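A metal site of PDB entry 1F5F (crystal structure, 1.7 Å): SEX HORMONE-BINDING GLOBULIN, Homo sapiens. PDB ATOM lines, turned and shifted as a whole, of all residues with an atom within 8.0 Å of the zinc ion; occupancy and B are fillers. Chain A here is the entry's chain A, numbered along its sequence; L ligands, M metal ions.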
ATOM      1  N   THR A  60      14.794  16.000   8.937  1.00  0.00           N
ATOM      2  CA  THR A  60      15.832  16.586   8.065  1.00  0.00           C
ATOM      3  C   THR A  60      17.067  15.809   8.529  1.00  0.00           C
ATOM      4  O   THR A  60      18.109  15.799   7.890  1.00  0.00           O
ATOM      5  CB  THR A  60      16.084  18.085   8.103  1.00  0.00           C
ATOM      6  OG1 THR A  60      16.231  18.674   9.407  1.00  0.00           O
ATOM      7  CG2 THR A  60      14.924  18.844   7.467  1.00  0.00           C
ATOM      8  N   ASN A  61      16.864  15.112   9.637  1.00  0.00           N
ATOM      9  CA  ASN A  61      17.846  14.267  10.318  1.00  0.00           C
ATOM     10  C   ASN A  61      17.106  13.433  11.371  1.00  0.00           C
ATOM     11  O   ASN A  61      16.299  13.968  12.136  1.00  0.00           O
ATOM     12  CB  ASN A  61      18.880  15.180  10.976  1.00  0.00           C
ATOM     13  CG  ASN A  61      20.174  14.481  11.322  1.00  0.00           C
ATOM     14  OD1 ASN A  61      20.141  13.494  12.081  1.00  0.00           O
ATOM     15  ND2 ASN A  61      21.287  14.957  10.754  1.00  0.00           N
ATOM     16  N   LYS A  63      18.260  11.591  13.840  1.00  0.00           N
ATOM     17  CA  LYS A  63      18.776  11.806  15.200  1.00  0.00           C
ATOM     18  C   LYS A  63      18.506  13.234  15.665  1.00  0.00           C
ATOM     19  O   LYS A  63      17.886  13.507  16.701  1.00  0.00           O
ATOM     20  CB  LYS A  63      20.248  11.415  15.207  1.00  0.00           C
ATOM     21  CG  LYS A  63      21.239  12.399  15.794  1.00  0.00           C
ATOM     22  CD  LYS A  63      22.370  11.709  16.537  1.00  0.00           C
ATOM     23  CE  LYS A  63      22.720  12.423  17.831  1.00  0.00           C
ATOM     24  NZ  LYS A  63      23.521  11.557  18.742  1.00  0.00           N
ATOM     25  N   ASP A  64      18.719  14.208  14.776  1.00  0.00           N
ATOM     26  CA  ASP A  64      18.808  15.596  15.173  1.00  0.00           C
ATOM     27  C   ASP A  64      17.561  16.459  15.036  1.00  0.00           C
ATOM     28  O   ASP A  64      17.492  17.502  15.723  1.00  0.00           O
ATOM     29  CB  ASP A  64      19.937  16.227  14.319  1.00  0.00           C
ATOM     30  CG  ASP A  64      21.228  16.293  15.113  1.00  0.00           C
ATOM     31  OD1 ASP A  64      21.137  16.130  16.350  1.00  0.00           O
ATOM     32  OD2 ASP A  64      22.326  16.491  14.552  1.00  0.00           O
ATOM     33  N   ASP A  65      16.863  16.326  13.882  1.00  0.00           N
ATOM     34  CA  ASP A  65      15.879  17.353  13.550  1.00  0.00           C
ATOM     35  C   ASP A  65      14.660  16.613  12.986  1.00  0.00           C
ATOM     36  O   ASP A  65      14.612  16.176  11.830  1.00  0.00           O
ATOM     37  CB  ASP A  65      16.329  18.259  12.390  1.00  0.00           C
ATOM     38  CG  ASP A  65      17.657  18.996  12.522  1.00  0.00           C
ATOM     39  OD1 ASP A  65      18.662  18.262  12.481  1.00  0.00           O
ATOM     40  OD2 ASP A  65      17.598  20.213  12.707  1.00  0.00           O
ATOM     41  N   TRP A  66      13.677  16.399  13.879  1.00  0.00           N
ATOM     42  CA  TRP A  66      12.496  15.616  13.521  1.00  0.00           C
ATOM     43  C   TRP A  66      11.212  16.179  14.077  1.00  0.00           C
ATOM     44  O   TRP A  66      11.214  17.047  14.969  1.00  0.00           O
ATOM     45  CB  TRP A  66      12.775  14.127  13.835  1.00  0.00           C
ATOM     46  CG  TRP A  66      12.918  13.798  15.285  1.00  0.00           C
ATOM     47  CD1 TRP A  66      14.092  13.742  15.973  1.00  0.00           C
ATOM     48  CD2 TRP A  66      11.869  13.608  16.256  1.00  0.00           C
ATOM     49  NE1 TRP A  66      13.860  13.464  17.319  1.00  0.00           N
ATOM     50  CE2 TRP A  66      12.504  13.369  17.475  1.00  0.00           C
ATOM     51  CE3 TRP A  66      10.479  13.606  16.155  1.00  0.00           C
ATOM     52  CZ2 TRP A  66      11.765  13.160  18.671  1.00  0.00           C
ATOM     53  CZ3 TRP A  66       9.733  13.365  17.326  1.00  0.00           C
ATOM     54  CH2 TRP A  66      10.403  13.150  18.533  1.00  0.00           C
ATOM     55  N   HIS A  81      11.786  17.866  17.735  1.00  0.00           N
ATOM     56  CA  HIS A  81      13.115  17.959  18.254  1.00  0.00           C
ATOM     57  C   HIS A  81      14.047  18.540  17.202  1.00  0.00           C
ATOM     58  O   HIS A  81      14.219  17.880  16.163  1.00  0.00           O
ATOM     59  CB  HIS A  81      13.539  16.577  18.784  1.00  0.00           C
ATOM     60  CG  HIS A  81      14.944  16.563  19.255  1.00  0.00           C
ATOM     61  ND1 HIS A  81      15.208  16.350  20.593  1.00  0.00           N
ATOM     62  CD2 HIS A  81      16.155  16.616  18.654  1.00  0.00           C
ATOM     63  CE1 HIS A  81      16.502  16.305  20.800  1.00  0.00           C
ATOM     64  NE2 HIS A  81      17.110  16.509  19.644  1.00  0.00           N
ATOM     65  N   ASN A  82      14.676  19.690  17.454  1.00  0.00           N
ATOM     66  CA  ASN A  82      15.593  20.277  16.478  1.00  0.00           C
ATOM     67  C   ASN A  82      16.544  21.162  17.285  1.00  0.00           C
ATOM     68  O   ASN A  82      16.574  21.117  18.511  1.00  0.00           O
ATOM     69  CB  ASN A  82      14.834  20.952  15.322  1.00  0.00           C
ATOM     70  CG  ASN A  82      14.009  22.168  15.698  1.00  0.00           C
ATOM     71  OD1 ASN A  82      14.296  22.768  16.728  1.00  0.00           O
ATOM     72  ND2 ASN A  82      13.068  22.614  14.873  1.00  0.00           N
ATOM     73  N   HIS A  83      17.338  21.955  16.556  1.00  0.00           N
ATOM     74  CA  HIS A  83      18.348  22.783  17.209  1.00  0.00           C
ATOM     75  C   HIS A  83      17.738  23.865  18.097  1.00  0.00           C
ATOM     76  O   HIS A  83      18.439  24.425  18.945  1.00  0.00           O
ATOM     77  CB  HIS A  83      19.166  23.502  16.103  1.00  0.00           C
ATOM     78  CG  HIS A  83      19.876  22.436  15.328  1.00  0.00           C
ATOM     79  ND1 HIS A  83      20.904  21.679  15.858  1.00  0.00           N
ATOM     80  CD2 HIS A  83      19.614  21.918  14.099  1.00  0.00           C
ATOM     81  CE1 HIS A  83      21.317  20.779  14.981  1.00  0.00           C
ATOM     82  NE2 HIS A  83      20.504  20.882  13.947  1.00  0.00           N
ATOM     83  N   TRP A  84      16.514  24.254  17.832  1.00  0.00           N
ATOM     84  CA  TRP A  84      15.880  25.391  18.500  1.00  0.00           C
ATOM     85  C   TRP A  84      14.933  24.919  19.605  1.00  0.00           C
ATOM     86  O   TRP A  84      14.701  25.732  20.525  1.00  0.00           O
ATOM     87  CB  TRP A  84      15.066  26.276  17.561  1.00  0.00           C
ATOM     88  CG  TRP A  84      15.967  26.861  16.516  1.00  0.00           C
ATOM     89  CD1 TRP A  84      16.784  27.953  16.633  1.00  0.00           C
ATOM     90  CD2 TRP A  84      16.341  26.206  15.290  1.00  0.00           C
ATOM     91  NE1 TRP A  84      17.573  28.071  15.520  1.00  0.00           N
ATOM     92  CE2 TRP A  84      17.352  26.995  14.701  1.00  0.00           C
ATOM     93  CE3 TRP A  84      15.963  24.991  14.697  1.00  0.00           C
ATOM     94  CZ2 TRP A  84      17.927  26.660  13.469  1.00  0.00           C
ATOM     95  CZ3 TRP A  84      16.496  24.706  13.440  1.00  0.00           C
ATOM     96  CH2 TRP A  84      17.511  25.499  12.880  1.00  0.00           C
ATOM     97  N   HIS A 136      21.494  20.541   5.929  1.00  0.00           N
ATOM     98  CA  HIS A 136      20.247  19.761   5.886  1.00  0.00           C
ATOM     99  C   HIS A 136      19.673  19.822   4.475  1.00  0.00           C
ATOM    100  O   HIS A 136      18.783  20.602   4.123  1.00  0.00           O
ATOM    101  CB  HIS A 136      19.266  20.341   6.908  1.00  0.00           C
ATOM    102  CG  HIS A 136      19.808  20.655   8.271  1.00  0.00           C
ATOM    103  ND1 HIS A 136      20.680  21.704   8.509  1.00  0.00           N
ATOM    104  CD2 HIS A 136      19.540  20.115   9.478  1.00  0.00           C
ATOM    105  CE1 HIS A 136      20.875  21.815   9.815  1.00  0.00           C
ATOM    106  NE2 HIS A 136      20.157  20.893  10.441  1.00  0.00           N
HETATM  107  C1  LIG L   1       6.667  22.091   8.333  1.00  0.00           C
HETATM  108  C2  LIG L   1       5.275  22.100   7.697  1.00  0.00           C
HETATM  109  C3  LIG L   1       5.005  20.782   7.003  1.00  0.00           C
HETATM  110  O1  LIG L   1       4.348  20.750   5.971  1.00  0.00           O
HETATM  111  C4  LIG L   1       5.537  19.507   7.535  1.00  0.00           C
HETATM  112  C5  LIG L   1       6.929  19.585   8.135  1.00  0.00           C
HETATM  113  C6  LIG L   1       7.384  18.335   8.846  1.00  0.00           C
HETATM  114  C7  LIG L   1       8.886  18.308   9.141  1.00  0.00           C
HETATM  115  C8  LIG L   1       9.215  19.557  10.026  1.00  0.00           C
HETATM  116  C9  LIG L   1       8.647  20.817   9.372  1.00  0.00           C
HETATM  117  C10 LIG L   1       7.123  20.826   9.082  1.00  0.00           C
HETATM  118  C11 LIG L   1       9.052  22.093  10.144  1.00  0.00           C
HETATM  119  C12 LIG L   1      10.522  22.166  10.519  1.00  0.00           C
HETATM  120  C13 LIG L   1      11.078  20.908  11.133  1.00  0.00           C
HETATM  121  C14 LIG L   1      10.710  19.705  10.248  1.00  0.00           C
HETATM  122  C15 LIG L   1      11.459  18.544  10.943  1.00  0.00           C
HETATM  123  C16 LIG L   1      12.791  19.199  11.382  1.00  0.00           C
HETATM  124  C17 LIG L   1      12.568  20.702  11.194  1.00  0.00           C
HETATM  125  O2  LIG L   1      13.224  21.479  12.216  1.00  0.00           O
HETATM  126  C18 LIG L   1      10.505  20.781  12.583  1.00  0.00           C
HETATM  127  C19 LIG L   1       6.242  20.664  10.330  1.00  0.00           C
HETATM  128 ZN    ZN M   1      20.194  19.775  12.260  1.00  0.00          ZN
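The zinc ion is bound by NE2 of His 83, NE2 of His 136 and OD1 of Asp 65.
The zinc ion has three donor atoms within binding distance.
Slightly farther from the zinc ion lies the side-chain carboxylate (OD2) of Asp 65 (2.7 Å).
An oxygen (O2) of the ligand lies within hydrogen-bond range of the side-chain amide nitrogen (ND2) of Asn 82 (2.9 Å).
O of Asp 65 sits at hydrogen-bond distance from N of Thr 60.
Of the 11 residues printed, 3 come within 4 Å of the zinc ion.
Along chain A the residues within 4 Å of the zinc ion span positions 65 to 136.
The nearest printed residue that does not touch the zinc ion is Asp 64 (4.1 Å).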
